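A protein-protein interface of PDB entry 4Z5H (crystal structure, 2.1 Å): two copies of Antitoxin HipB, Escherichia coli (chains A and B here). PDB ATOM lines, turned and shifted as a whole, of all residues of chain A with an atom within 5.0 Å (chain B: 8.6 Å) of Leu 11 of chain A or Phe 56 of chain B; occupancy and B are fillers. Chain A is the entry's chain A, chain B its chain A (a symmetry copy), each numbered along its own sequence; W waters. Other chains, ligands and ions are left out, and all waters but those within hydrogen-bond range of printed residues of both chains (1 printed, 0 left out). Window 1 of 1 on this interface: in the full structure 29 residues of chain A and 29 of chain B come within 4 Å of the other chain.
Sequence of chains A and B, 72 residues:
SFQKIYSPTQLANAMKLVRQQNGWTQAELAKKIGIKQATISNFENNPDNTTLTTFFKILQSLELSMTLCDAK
The backbone carbonyl oxygen (O) of Ile 5 of chain A sits at hydrogen-bond distance from the side-chain hydroxyl (OG) of Ser 65 of chain B (3.0 Å). The backbone NH of Ile 5 of chain A is in hydrogen-bond range of the backbone carbonyl oxygen of Met 66 of chain B, at 2.8 Å.
The backbone NH (N) of Tyr 6 of chain A sits at hydrogen-bond distance from the side-chain amide oxygen (OE1) of Gln 10 of chain A. The side-chain hydroxyl of Ser 7 of chain A sits at hydrogen-bond distance from the backbone NH of Gln 10 of chain A (3.3 Å).
CD1 of Phe 56 of chain B touches C of Tyr 6 of chain A, at 3.3 Å. CE2 of Tyr 6 of chain A touches OG of Ser 65 of chain B, at 3.6 Å. N of Ser 7 of chain A touches CD1 of Phe 56 of chain B, 3.5 Å away. CG of Pro 8 of chain A touches C of Leu 52 of chain B (3.9 Å). N of Thr 53 of chain B touches CG of Pro 8 of chain A, 3.9 Å away. Pro 8 of chain A touches Phe 56 of chain B (N to CD2, 3.5 Å). Phe 56 of chain B touches Leu 11 of chain A. CB of Ala 14 of chain A touches CD1 of Leu 68 of chain B, at 3.8 Å. Leu 52 of chain B touches Phe 43 of chain A (CD1 to CE1, 3.7 Å). Phe 55 of chain A touches Leu 52 of chain B.
Printed residues of chain B within 4 Å of Leu 11 of chain A: Phe 56. Printed residues of chain B within 4 Å of Pro 8 of chain A: Leu 52, Thr 53 and Phe 56. No residue of chain B comes within 4 Å of Ala 12 of chain A. Printed residues of chain A within 4 Å of Ser 65 of chain B: Ile 5 and Tyr 6. Printed residues of chain B within 4 Å of Phe 55 of chain A: Leu 52 (3.9 Å). Of the printed residues of chain A, Met 66 of chain B touches Ile 5. Of the printed residues of chain B, Ser 7 of chain A touches Phe 56 (3.5 Å). Of the printed residues of chain A, Thr 53 of chain B touches Pro 8 (3.9 Å). Leu 62 of chain B touches none of the printed residues of chain A. The nearest printed residue of chain B that does not touch Leu 11 of chain A is Leu 68 of chain B (4.004 Å). The nearest printed residue of chain A that does not touch Thr 53 of chain B is Ser 7 of chain A (7.0 Å).
Hydrophobic or aromatic side chains of chain A within 4 Å of the printed part of chain B: Ile 5, Tyr 6, Pro 8, Leu 11, Ala 14, Phe 43 and Phe 55. Hydrophobic or aromatic side chains of chain B within 4 Å of the printed part of chain A: Leu 52, Phe 56, Met 66 and Leu 68. Among the printed residues, 13 pairs touch across the chains. Among the printed residues, no Asp or Glu carboxylate lies within 4 Å of a Lys or Arg side-chain nitrogen of the other chain.
Positions printed for both chains: 11, 15, 43 and 55.
Water W1 lies within hydrogen-bond range of O of Tyr 6 of chain A (2.9 Å) and O of Phe 56 of chain B (2.9 Å).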
ATOM      1  N   ILE A   5      -6.743 -12.560  -4.546  1.00  0.00           N
ATOM      2  CA  ILE A   5      -5.737 -12.819  -5.556  1.00  0.00           C
ATOM      3  C   ILE A   5      -6.286 -13.757  -6.637  1.00  0.00           C
ATOM      4  O   ILE A   5      -6.933 -14.737  -6.327  1.00  0.00           O
ATOM      5  CB  ILE A   5      -4.458 -13.377  -4.897  1.00  0.00           C
ATOM      6  CG1 ILE A   5      -3.884 -12.299  -3.975  1.00  0.00           C
ATOM      7  CG2 ILE A   5      -3.460 -13.895  -5.925  1.00  0.00           C
ATOM      8  CD1 ILE A   5      -2.888 -12.774  -2.976  1.00  0.00           C
ATOM      9  N   TYR A   6      -6.058 -13.395  -7.891  1.00  0.00           N
ATOM     10  CA  TYR A   6      -6.612 -14.077  -9.038  1.00  0.00           C
ATOM     11  C   TYR A   6      -5.621 -14.670 -10.042  1.00  0.00           C
ATOM     12  O   TYR A   6      -6.018 -15.265 -10.993  1.00  0.00           O
ATOM     13  CB  TYR A   6      -7.585 -13.154  -9.764  1.00  0.00           C
ATOM     14  CG  TYR A   6      -8.710 -12.643  -8.905  1.00  0.00           C
ATOM     15  CD1 TYR A   6      -8.539 -11.548  -8.085  1.00  0.00           C
ATOM     16  CD2 TYR A   6      -9.938 -13.262  -8.908  1.00  0.00           C
ATOM     17  CE1 TYR A   6      -9.562 -11.080  -7.312  1.00  0.00           C
ATOM     18  CE2 TYR A   6     -10.961 -12.808  -8.129  1.00  0.00           C
ATOM     19  CZ  TYR A   6     -10.768 -11.713  -7.333  1.00  0.00           C
ATOM     20  OH  TYR A   6     -11.764 -11.264  -6.552  1.00  0.00           O
ATOM     21  N   SER A   7      -4.335 -14.462  -9.836  1.00  0.00           N
ATOM     22  CA  SER A   7      -3.333 -14.989 -10.740  1.00  0.00           C
ATOM     23  C   SER A   7      -1.967 -15.247 -10.112  1.00  0.00           C
ATOM     24  O   SER A   7      -1.630 -14.714  -9.084  1.00  0.00           O
ATOM     25  CB  SER A   7      -3.157 -14.089 -11.969  1.00  0.00           C
ATOM     26  OG  SER A   7      -2.434 -12.923 -11.667  1.00  0.00           O
ATOM     27  N   PRO A   8      -1.146 -16.027 -10.803  1.00  0.00           N
ATOM     28  CA  PRO A   8       0.199 -16.291 -10.299  1.00  0.00           C
ATOM     29  C   PRO A   8       0.995 -14.984 -10.157  1.00  0.00           C
ATOM     30  O   PRO A   8       1.617 -14.819  -9.157  1.00  0.00           O
ATOM     31  CB  PRO A   8       0.811 -17.197 -11.361  1.00  0.00           C
ATOM     32  CG  PRO A   8      -0.355 -17.816 -12.040  1.00  0.00           C
ATOM     33  CD  PRO A   8      -1.392 -16.750 -12.054  1.00  0.00           C
ATOM     34  N   THR A   9       0.898 -14.066 -11.104  1.00  0.00           N
ATOM     35  CA  THR A   9       1.598 -12.798 -11.006  1.00  0.00           C
ATOM     36  C   THR A   9       1.159 -11.975  -9.787  1.00  0.00           C
ATOM     37  O   THR A   9       1.985 -11.493  -9.057  1.00  0.00           O
ATOM     38  CB  THR A   9       1.391 -11.948 -12.276  1.00  0.00           C
ATOM     39  OG1 THR A   9       1.961 -12.611 -13.392  1.00  0.00           O
ATOM     40  CG2 THR A   9       2.013 -10.568 -12.119  1.00  0.00           C
ATOM     41  N   GLN A  10      -0.138 -11.881  -9.564  1.00  0.00           N
ATOM     42  CA  GLN A  10      -0.681 -11.192  -8.417  1.00  0.00           C
ATOM     43  C   GLN A  10      -0.215 -11.866  -7.129  1.00  0.00           C
ATOM     44  O   GLN A  10       0.138 -11.208  -6.191  1.00  0.00           O
ATOM     45  CB  GLN A  10      -2.206 -11.170  -8.469  1.00  0.00           C
ATOM     46  CG  GLN A  10      -2.812 -10.224  -9.483  1.00  0.00           C
ATOM     47  CD  GLN A  10      -4.315 -10.353  -9.602  1.00  0.00           C
ATOM     48  OE1 GLN A  10      -4.975 -10.859  -8.737  1.00  0.00           O
ATOM     49  NE2 GLN A  10      -4.843  -9.876 -10.692  1.00  0.00           N
ATOM     50  N   LEU A  11      -0.203 -13.186  -7.132  1.00  0.00           N
ATOM     51  CA  LEU A  11       0.233 -13.944  -5.986  1.00  0.00           C
ATOM     52  C   LEU A  11       1.703 -13.683  -5.655  1.00  0.00           C
ATOM     53  O   LEU A  11       2.037 -13.444  -4.522  1.00  0.00           O
ATOM     54  CB  LEU A  11       0.016 -15.430  -6.225  1.00  0.00           C
ATOM     55  CG  LEU A  11       0.455 -16.395  -5.133  1.00  0.00           C
ATOM     56  CD1 LEU A  11      -0.062 -16.039  -3.757  1.00  0.00           C
ATOM     57  CD2 LEU A  11       0.142 -17.832  -5.509  1.00  0.00           C
ATOM     58  N   ALA A  12       2.546 -13.736  -6.674  1.00  0.00           N
ATOM     59  CA  ALA A  12       3.971 -13.510  -6.524  1.00  0.00           C
ATOM     60  C   ALA A  12       4.274 -12.084  -6.052  1.00  0.00           C
ATOM     61  O   ALA A  12       5.081 -11.889  -5.186  1.00  0.00           O
ATOM     62  CB  ALA A  12       4.701 -13.808  -7.819  1.00  0.00           C
ATOM     63  N   ASN A  13       3.583 -11.106  -6.620  1.00  0.00           N
ATOM     64  CA  ASN A  13       3.769  -9.727  -6.245  1.00  0.00           C
ATOM     65  C   ASN A  13       3.411  -9.521  -4.777  1.00  0.00           C
ATOM     66  O   ASN A  13       4.140  -8.879  -4.073  1.00  0.00           O
ATOM     67  CB  ASN A  13       2.919  -8.795  -7.111  1.00  0.00           C
ATOM     68  CG  ASN A  13       3.412  -8.696  -8.545  1.00  0.00           C
ATOM     69  OD1 ASN A  13       4.431  -9.221  -8.879  1.00  0.00           O
ATOM     70  ND2 ASN A  13       2.675  -8.033  -9.374  1.00  0.00           N
ATOM     71  N   ALA A  14       2.302 -10.099  -4.328  1.00  0.00           N
ATOM     72  CA  ALA A  14       1.906 -10.012  -2.933  1.00  0.00           C
ATOM     73  C   ALA A  14       2.899 -10.667  -1.959  1.00  0.00           C
ATOM     74  O   ALA A  14       3.195 -10.142  -0.922  1.00  0.00           O
ATOM     75  CB  ALA A  14       0.533 -10.610  -2.734  1.00  0.00           C
ATOM     76  N   MET A  15       3.380 -11.839  -2.315  1.00  0.00           N
ATOM     77  CA  MET A  15       4.358 -12.532  -1.514  1.00  0.00           C
ATOM     78  C   MET A  15       5.729 -11.858  -1.428  1.00  0.00           C
ATOM     79  O   MET A  15       6.343 -11.880  -0.401  1.00  0.00           O
ATOM     80  CB  MET A  15       4.441 -13.989  -1.892  1.00  0.00           C
ATOM     81  CG  MET A  15       3.183 -14.717  -1.483  1.00  0.00           C
ATOM     82  SD  MET A  15       3.029 -16.339  -2.173  1.00  0.00           S
ATOM     83  CE  MET A  15       4.209 -17.214  -1.189  1.00  0.00           C
ATOM     84  N   PHE A  43      10.139 -17.765  -8.756  1.00  0.00           N
ATOM     85  CA  PHE A  43       8.765 -17.611  -8.324  1.00  0.00           C
ATOM     86  C   PHE A  43       8.330 -16.145  -8.378  1.00  0.00           C
ATOM     87  O   PHE A  43       7.297 -15.847  -8.905  1.00  0.00           O
ATOM     88  CB  PHE A  43       8.564 -18.154  -6.902  1.00  0.00           C
ATOM     89  CG  PHE A  43       7.287 -17.697  -6.235  1.00  0.00           C
ATOM     90  CD1 PHE A  43       6.060 -18.137  -6.678  1.00  0.00           C
ATOM     91  CD2 PHE A  43       7.319 -16.791  -5.206  1.00  0.00           C
ATOM     92  CE1 PHE A  43       4.896 -17.701  -6.071  1.00  0.00           C
ATOM     93  CE2 PHE A  43       6.169 -16.361  -4.588  1.00  0.00           C
ATOM     94  CZ  PHE A  43       4.952 -16.813  -5.018  1.00  0.00           C
ATOM     95  N   PHE A  55       5.269 -23.088  -3.960  1.00  0.00           N
ATOM     96  CA  PHE A  55       4.444 -22.029  -3.425  1.00  0.00           C
ATOM     97  C   PHE A  55       4.191 -22.234  -1.927  1.00  0.00           C
ATOM     98  O   PHE A  55       4.428 -21.339  -1.160  1.00  0.00           O
ATOM     99  CB  PHE A  55       3.123 -21.991  -4.196  1.00  0.00           C
ATOM    100  CG  PHE A  55       1.995 -21.295  -3.484  1.00  0.00           C
ATOM    101  CD1 PHE A  55       2.147 -20.029  -2.961  1.00  0.00           C
ATOM    102  CD2 PHE A  55       0.778 -21.918  -3.342  1.00  0.00           C
ATOM    103  CE1 PHE A  55       1.110 -19.400  -2.325  1.00  0.00           C
ATOM    104  CE2 PHE A  55      -0.274 -21.295  -2.701  1.00  0.00           C
ATOM    105  CZ  PHE A  55      -0.103 -20.032  -2.191  1.00  0.00           C
ATOM    106  N   LEU B  11      -4.964 -28.237  -0.303  1.00  0.00           N
ATOM    107  CA  LEU B  11      -5.557 -27.352  -1.275  1.00  0.00           C
ATOM    108  C   LEU B  11      -6.430 -28.106  -2.278  1.00  0.00           C
ATOM    109  O   LEU B  11      -7.538 -27.705  -2.541  1.00  0.00           O
ATOM    110  CB  LEU B  11      -4.473 -26.584  -2.015  1.00  0.00           C
ATOM    111  CG  LEU B  11      -4.907 -25.622  -3.112  1.00  0.00           C
ATOM    112  CD1 LEU B  11      -5.988 -24.656  -2.685  1.00  0.00           C
ATOM    113  CD2 LEU B  11      -3.713 -24.913  -3.729  1.00  0.00           C
ATOM    114  N   MET B  15     -10.554 -27.923  -2.859  1.00  0.00           N
ATOM    115  CA  MET B  15     -11.094 -27.594  -4.155  1.00  0.00           C
ATOM    116  C   MET B  15     -11.981 -28.670  -4.787  1.00  0.00           C
ATOM    117  O   MET B  15     -12.950 -28.352  -5.413  1.00  0.00           O
ATOM    118  CB  MET B  15     -10.018 -27.097  -5.085  1.00  0.00           C
ATOM    119  CG  MET B  15      -9.513 -25.745  -4.642  1.00  0.00           C
ATOM    120  SD  MET B  15      -8.029 -25.223  -5.454  1.00  0.00           S
ATOM    121  CE  MET B  15      -8.671 -24.794  -7.044  1.00  0.00           C
ATOM    122  N   ILE B  33     -12.636 -23.468 -18.782  1.00  0.00           N
ATOM    123  CA  ILE B  33     -11.366 -22.774 -18.688  1.00  0.00           C
ATOM    124  C   ILE B  33     -10.332 -23.142 -19.745  1.00  0.00           C
ATOM    125  O   ILE B  33      -9.221 -22.692 -19.686  1.00  0.00           O
ATOM    126  CB  ILE B  33     -10.746 -22.910 -17.284  1.00  0.00           C
ATOM    127  CG1 ILE B  33     -10.480 -24.371 -16.948  1.00  0.00           C
ATOM    128  CG2 ILE B  33     -11.629 -22.250 -16.245  1.00  0.00           C
ATOM    129  CD1 ILE B  33      -9.895 -24.571 -15.577  1.00  0.00           C
ATOM    130  N   ILE B  35      -8.723 -26.157 -20.503  1.00  0.00           N
ATOM    131  CA  ILE B  35      -7.647 -27.066 -20.169  1.00  0.00           C
ATOM    132  C   ILE B  35      -8.180 -28.489 -20.230  1.00  0.00           C
ATOM    133  O   ILE B  35      -9.361 -28.686 -20.359  1.00  0.00           O
ATOM    134  CB  ILE B  35      -7.004 -26.789 -18.798  1.00  0.00           C
ATOM    135  CG1 ILE B  35      -7.956 -27.153 -17.663  1.00  0.00           C
ATOM    136  CG2 ILE B  35      -6.507 -25.365 -18.707  1.00  0.00           C
ATOM    137  CD1 ILE B  35      -7.343 -27.036 -16.296  1.00  0.00           C
ATOM    138  N   PHE B  43      -4.512 -32.597 -10.857  1.00  0.00           N
ATOM    139  CA  PHE B  43      -4.483 -31.639  -9.772  1.00  0.00           C
ATOM    140  C   PHE B  43      -5.122 -32.216  -8.505  1.00  0.00           C
ATOM    141  O   PHE B  43      -4.553 -32.130  -7.456  1.00  0.00           O
ATOM    142  CB  PHE B  43      -5.199 -30.336 -10.160  1.00  0.00           C
ATOM    143  CG  PHE B  43      -5.550 -29.446  -8.990  1.00  0.00           C
ATOM    144  CD1 PHE B  43      -4.568 -28.802  -8.269  1.00  0.00           C
ATOM    145  CD2 PHE B  43      -6.853 -29.300  -8.586  1.00  0.00           C
ATOM    146  CE1 PHE B  43      -4.898 -28.001  -7.192  1.00  0.00           C
ATOM    147  CE2 PHE B  43      -7.191 -28.496  -7.523  1.00  0.00           C
ATOM    148  CZ  PHE B  43      -6.217 -27.843  -6.821  1.00  0.00           C
ATOM    149  N   THR B  50       1.779 -29.589  -9.700  1.00  0.00           N
ATOM    150  CA  THR B  50       0.849 -28.777 -10.455  1.00  0.00           C
ATOM    151  C   THR B  50       1.303 -27.301 -10.499  1.00  0.00           C
ATOM    152  O   THR B  50       1.777 -26.775  -9.537  1.00  0.00           O
ATOM    153  CB  THR B  50      -0.555 -28.870  -9.831  1.00  0.00           C
ATOM    154  OG1 THR B  50      -1.046 -30.193  -9.982  1.00  0.00           O
ATOM    155  CG2 THR B  50      -1.510 -27.931 -10.502  1.00  0.00           C
ATOM    156  N   THR B  51       1.189 -26.681 -11.653  1.00  0.00           N
ATOM    157  CA  THR B  51       1.575 -25.292 -11.820  1.00  0.00           C
ATOM    158  C   THR B  51       0.597 -24.270 -11.225  1.00  0.00           C
ATOM    159  O   THR B  51      -0.581 -24.519 -11.116  1.00  0.00           O
ATOM    160  CB  THR B  51       1.825 -24.931 -13.290  1.00  0.00           C
ATOM    161  OG1 THR B  51       0.600 -24.961 -14.015  1.00  0.00           O
ATOM    162  CG2 THR B  51       2.845 -25.864 -13.908  1.00  0.00           C
ATOM    163  N   LEU B  52       1.113 -23.106 -10.899  1.00  0.00           N
ATOM    164  CA  LEU B  52       0.327 -22.038 -10.336  1.00  0.00           C
ATOM    165  C   LEU B  52      -0.765 -21.639 -11.342  1.00  0.00           C
ATOM    166  O   LEU B  52      -1.859 -21.349 -10.948  1.00  0.00           O
ATOM    167  CB  LEU B  52       1.192 -20.844  -9.943  1.00  0.00           C
ATOM    168  CG  LEU B  52       2.046 -20.977  -8.686  1.00  0.00           C
ATOM    169  CD1 LEU B  52       2.758 -19.714  -8.301  1.00  0.00           C
ATOM    170  CD2 LEU B  52       1.232 -21.493  -7.518  1.00  0.00           C
ATOM    171  N   THR B  53      -0.431 -21.651 -12.625  1.00  0.00           N
ATOM    172  CA  THR B  53      -1.368 -21.306 -13.672  1.00  0.00           C
ATOM    173  C   THR B  53      -2.561 -22.263 -13.687  1.00  0.00           C
ATOM    174  O   THR B  53      -3.684 -21.837 -13.751  1.00  0.00           O
ATOM    175  CB  THR B  53      -0.689 -21.297 -15.063  1.00  0.00           C
ATOM    176  OG1 THR B  53       0.226 -20.210 -15.135  1.00  0.00           O
ATOM    177  CG2 THR B  53      -1.695 -21.150 -16.166  1.00  0.00           C
ATOM    178  N   THR B  54      -2.295 -23.547 -13.592  1.00  0.00           N
ATOM    179  CA  THR B  54      -3.368 -24.511 -13.541  1.00  0.00           C
ATOM    180  C   THR B  54      -4.238 -24.250 -12.309  1.00  0.00           C
ATOM    181  O   THR B  54      -5.434 -24.216 -12.415  1.00  0.00           O
ATOM    182  CB  THR B  54      -2.840 -25.950 -13.545  1.00  0.00           C
ATOM    183  OG1 THR B  54      -2.268 -26.240 -14.818  1.00  0.00           O
ATOM    184  CG2 THR B  54      -3.946 -26.928 -13.253  1.00  0.00           C
ATOM    185  N   PHE B  55      -3.613 -23.987 -11.173  1.00  0.00           N
ATOM    186  CA  PHE B  55      -4.346 -23.755  -9.951  1.00  0.00           C
ATOM    187  C   PHE B  55      -5.293 -22.558 -10.096  1.00  0.00           C
ATOM    188  O   PHE B  55      -6.455 -22.686  -9.818  1.00  0.00           O
ATOM    189  CB  PHE B  55      -3.352 -23.522  -8.812  1.00  0.00           C
ATOM    190  CG  PHE B  55      -3.919 -22.814  -7.612  1.00  0.00           C
ATOM    191  CD1 PHE B  55      -5.076 -23.250  -7.001  1.00  0.00           C
ATOM    192  CD2 PHE B  55      -3.285 -21.709  -7.097  1.00  0.00           C
ATOM    193  CE1 PHE B  55      -5.578 -22.604  -5.900  1.00  0.00           C
ATOM    194  CE2 PHE B  55      -3.782 -21.051  -5.990  1.00  0.00           C
ATOM    195  CZ  PHE B  55      -4.933 -21.500  -5.395  1.00  0.00           C
ATOM    196  N   PHE B  56      -4.799 -21.430 -10.592  1.00  0.00           N
ATOM    197  CA  PHE B  56      -5.636 -20.252 -10.740  1.00  0.00           C
ATOM    198  C   PHE B  56      -6.798 -20.420 -11.721  1.00  0.00           C
ATOM    199  O   PHE B  56      -7.852 -19.915 -11.496  1.00  0.00           O
ATOM    200  CB  PHE B  56      -4.832 -18.970 -10.954  1.00  0.00           C
ATOM    201  CG  PHE B  56      -4.258 -18.417  -9.685  1.00  0.00           C
ATOM    202  CD1 PHE B  56      -5.039 -17.689  -8.811  1.00  0.00           C
ATOM    203  CD2 PHE B  56      -2.950 -18.671  -9.340  1.00  0.00           C
ATOM    204  CE1 PHE B  56      -4.523 -17.211  -7.630  1.00  0.00           C
ATOM    205  CE2 PHE B  56      -2.420 -18.191  -8.160  1.00  0.00           C
ATOM    206  CZ  PHE B  56      -3.205 -17.469  -7.301  1.00  0.00           C
ATOM    207  N   LYS B  57      -6.568 -21.146 -12.794  1.00  0.00           N
ATOM    208  CA  LYS B  57      -7.598 -21.419 -13.767  1.00  0.00           C
ATOM    209  C   LYS B  57      -8.741 -22.242 -13.169  1.00  0.00           C
ATOM    210  O   LYS B  57      -9.884 -21.920 -13.346  1.00  0.00           O
ATOM    211  CB  LYS B  57      -7.008 -22.104 -14.986  1.00  0.00           C
ATOM    212  CG  LYS B  57      -6.203 -21.162 -15.855  1.00  0.00           C
ATOM    213  CD  LYS B  57      -5.676 -21.836 -17.096  1.00  0.00           C
ATOM    214  CE  LYS B  57      -5.020 -20.825 -18.011  1.00  0.00           C
ATOM    215  NZ  LYS B  57      -4.388 -21.510 -19.140  1.00  0.00           N
ATOM    216  N   ILE B  58      -8.381 -23.286 -12.436  1.00  0.00           N
ATOM    217  CA  ILE B  58      -9.343 -24.125 -11.745  1.00  0.00           C
ATOM    218  C   ILE B  58     -10.108 -23.317 -10.696  1.00  0.00           C
ATOM    219  O   ILE B  58     -11.303 -23.418 -10.601  1.00  0.00           O
ATOM    220  CB  ILE B  58      -8.703 -25.398 -11.152  1.00  0.00           C
ATOM    221  CG1 ILE B  58      -8.175 -26.288 -12.275  1.00  0.00           C
ATOM    222  CG2 ILE B  58      -9.715 -26.185 -10.355  1.00  0.00           C
ATOM    223  CD1 ILE B  58      -7.275 -27.407 -11.838  1.00  0.00           C
ATOM    224  N   LEU B  59      -9.408 -22.447  -9.986  1.00  0.00           N
ATOM    225  CA  LEU B  59     -10.032 -21.614  -8.993  1.00  0.00           C
ATOM    226  C   LEU B  59     -11.114 -20.771  -9.646  1.00  0.00           C
ATOM    227  O   LEU B  59     -12.197 -20.701  -9.138  1.00  0.00           O
ATOM    228  CB  LEU B  59      -9.012 -20.650  -8.414  1.00  0.00           C
ATOM    229  CG  LEU B  59      -8.434 -20.686  -7.025  1.00  0.00           C
ATOM    230  CD1 LEU B  59      -7.802 -19.355  -6.679  1.00  0.00           C
ATOM    231  CD2 LEU B  59      -9.338 -21.203  -5.928  1.00  0.00           C
ATOM    232  N   GLN B  60     -10.813 -20.194 -10.802  1.00  0.00           N
ATOM    233  CA  GLN B  60     -11.774 -19.408 -11.548  1.00  0.00           C
ATOM    234  C   GLN B  60     -12.994 -20.244 -11.959  1.00  0.00           C
ATOM    235  O   GLN B  60     -14.107 -19.810 -11.790  1.00  0.00           O
ATOM    236  CB  GLN B  60     -11.142 -18.801 -12.796  1.00  0.00           C
ATOM    237  CG  GLN B  60     -12.070 -17.842 -13.515  1.00  0.00           C
ATOM    238  CD  GLN B  60     -11.803 -17.696 -15.001  1.00  0.00           C
ATOM    239  OE1 GLN B  60     -10.999 -18.407 -15.578  1.00  0.00           O
ATOM    240  NE2 GLN B  60     -12.462 -16.743 -15.612  1.00  0.00           N
ATOM    241  N   SER B  61     -12.748 -21.460 -12.410  1.00  0.00           N
ATOM    242  CA  SER B  61     -13.807 -22.361 -12.833  1.00  0.00           C
ATOM    243  C   SER B  61     -14.762 -22.664 -11.681  1.00  0.00           C
ATOM    244  O   SER B  61     -15.922 -22.846 -11.908  1.00  0.00           O
ATOM    245  CB  SER B  61     -13.265 -23.653 -13.450  1.00  0.00           C
ATOM    246  OG  SER B  61     -12.880 -24.575 -12.492  1.00  0.00           O
ATOM    247  N   LEU B  62     -14.244 -22.677 -10.461  1.00  0.00           N
ATOM    248  CA  LEU B  62     -15.000 -22.992  -9.277  1.00  0.00           C
ATOM    249  C   LEU B  62     -15.667 -21.757  -8.659  1.00  0.00           C
ATOM    250  O   LEU B  62     -16.219 -21.826  -7.598  1.00  0.00           O
ATOM    251  CB  LEU B  62     -14.131 -23.722  -8.253  1.00  0.00           C
ATOM    252  CG  LEU B  62     -13.597 -25.126  -8.547  1.00  0.00           C
ATOM    253  CD1 LEU B  62     -12.580 -25.570  -7.512  1.00  0.00           C
ATOM    254  CD2 LEU B  62     -14.714 -26.143  -8.657  1.00  0.00           C
ATOM    255  N   GLU B  63     -15.568 -20.628  -9.338  1.00  0.00           N
ATOM    256  CA  GLU B  63     -16.061 -19.348  -8.845  1.00  0.00           C
ATOM    257  C   GLU B  63     -15.404 -18.917  -7.521  1.00  0.00           C
ATOM    258  O   GLU B  63     -16.014 -18.308  -6.682  1.00  0.00           O
ATOM    259  CB  GLU B  63     -17.591 -19.363  -8.749  1.00  0.00           C
ATOM    260  CG  GLU B  63     -18.247 -19.729 -10.057  1.00  0.00           C
ATOM    261  CD  GLU B  63     -19.759 -19.872  -9.997  1.00  0.00           C
ATOM    262  OE1 GLU B  63     -20.323 -20.074  -8.918  1.00  0.00           O
ATOM    263  OE2 GLU B  63     -20.380 -19.807 -11.057  1.00  0.00           O
ATOM    264  N   LEU B  64     -14.138 -19.246  -7.389  1.00  0.00           N
ATOM    265  CA  LEU B  64     -13.348 -18.965  -6.221  1.00  0.00           C
ATOM    266  C   LEU B  64     -12.174 -18.047  -6.520  1.00  0.00           C
ATOM    267  O   LEU B  64     -11.710 -17.962  -7.626  1.00  0.00           O
ATOM    268  CB  LEU B  64     -12.782 -20.245  -5.622  1.00  0.00           C
ATOM    269  CG  LEU B  64     -13.719 -21.334  -5.114  1.00  0.00           C
ATOM    270  CD1 LEU B  64     -12.931 -22.573  -4.774  1.00  0.00           C
ATOM    271  CD2 LEU B  64     -14.508 -20.843  -3.934  1.00  0.00           C
ATOM    272  N   SER B  65     -11.697 -17.439  -5.459  1.00  0.00           N
ATOM    273  CA  SER B  65     -10.498 -16.654  -5.392  1.00  0.00           C
ATOM    274  C   SER B  65      -9.755 -17.182  -4.160  1.00  0.00           C
ATOM    275  O   SER B  65     -10.201 -18.120  -3.535  1.00  0.00           O
ATOM    276  CB  SER B  65     -10.833 -15.172  -5.242  1.00  0.00           C
ATOM    277  OG  SER B  65      -9.684 -14.390  -5.130  1.00  0.00           O
ATOM    278  N   MET B  66      -8.625 -16.579  -3.836  1.00  0.00           N
ATOM    279  CA  MET B  66      -7.877 -16.906  -2.641  1.00  0.00           C
ATOM    280  C   MET B  66      -7.271 -15.659  -2.027  1.00  0.00           C
ATOM    281  O   MET B  66      -7.097 -14.689  -2.711  1.00  0.00           O
ATOM    282  CB  MET B  66      -6.756 -17.866  -2.971  1.00  0.00           C
ATOM    283  CG  MET B  66      -5.776 -17.305  -3.984  1.00  0.00           C
ATOM    284  SD  MET B  66      -4.079 -17.632  -3.571  1.00  0.00           S
ATOM    285  CE  MET B  66      -3.872 -16.742  -2.077  1.00  0.00           C
ATOM    286  N   THR B  67      -6.941 -15.719  -0.748  1.00  0.00           N
ATOM    287  CA  THR B  67      -6.144 -14.694  -0.084  1.00  0.00           C
ATOM    288  C   THR B  67      -5.061 -15.306   0.794  1.00  0.00           C
ATOM    289  O   THR B  67      -5.174 -16.417   1.251  1.00  0.00           O
ATOM    290  CB  THR B  67      -6.971 -13.708   0.779  1.00  0.00           C
ATOM    291  OG1 THR B  67      -7.385 -14.341   1.983  1.00  0.00           O
ATOM    292  CG2 THR B  67      -8.174 -13.227   0.051  1.00  0.00           C
ATOM    293  N   LEU B  68      -4.015 -14.545   1.002  1.00  0.00           N
ATOM    294  CA  LEU B  68      -3.035 -14.831   2.009  1.00  0.00           C
ATOM    295  C   LEU B  68      -3.552 -14.508   3.401  1.00  0.00           C
ATOM    296  O   LEU B  68      -4.468 -13.745   3.561  1.00  0.00           O
ATOM    297  CB  LEU B  68      -1.755 -14.077   1.740  1.00  0.00           C
ATOM    298  CG  LEU B  68      -1.155 -14.226   0.356  1.00  0.00           C
ATOM    299  CD1 LEU B  68      -0.244 -13.067   0.041  1.00  0.00           C
ATOM    300  CD2 LEU B  68      -0.451 -15.545   0.197  1.00  0.00           C
HETATM  301  O   HOH W   1      -8.246 -17.134 -10.676  1.00  0.00           O
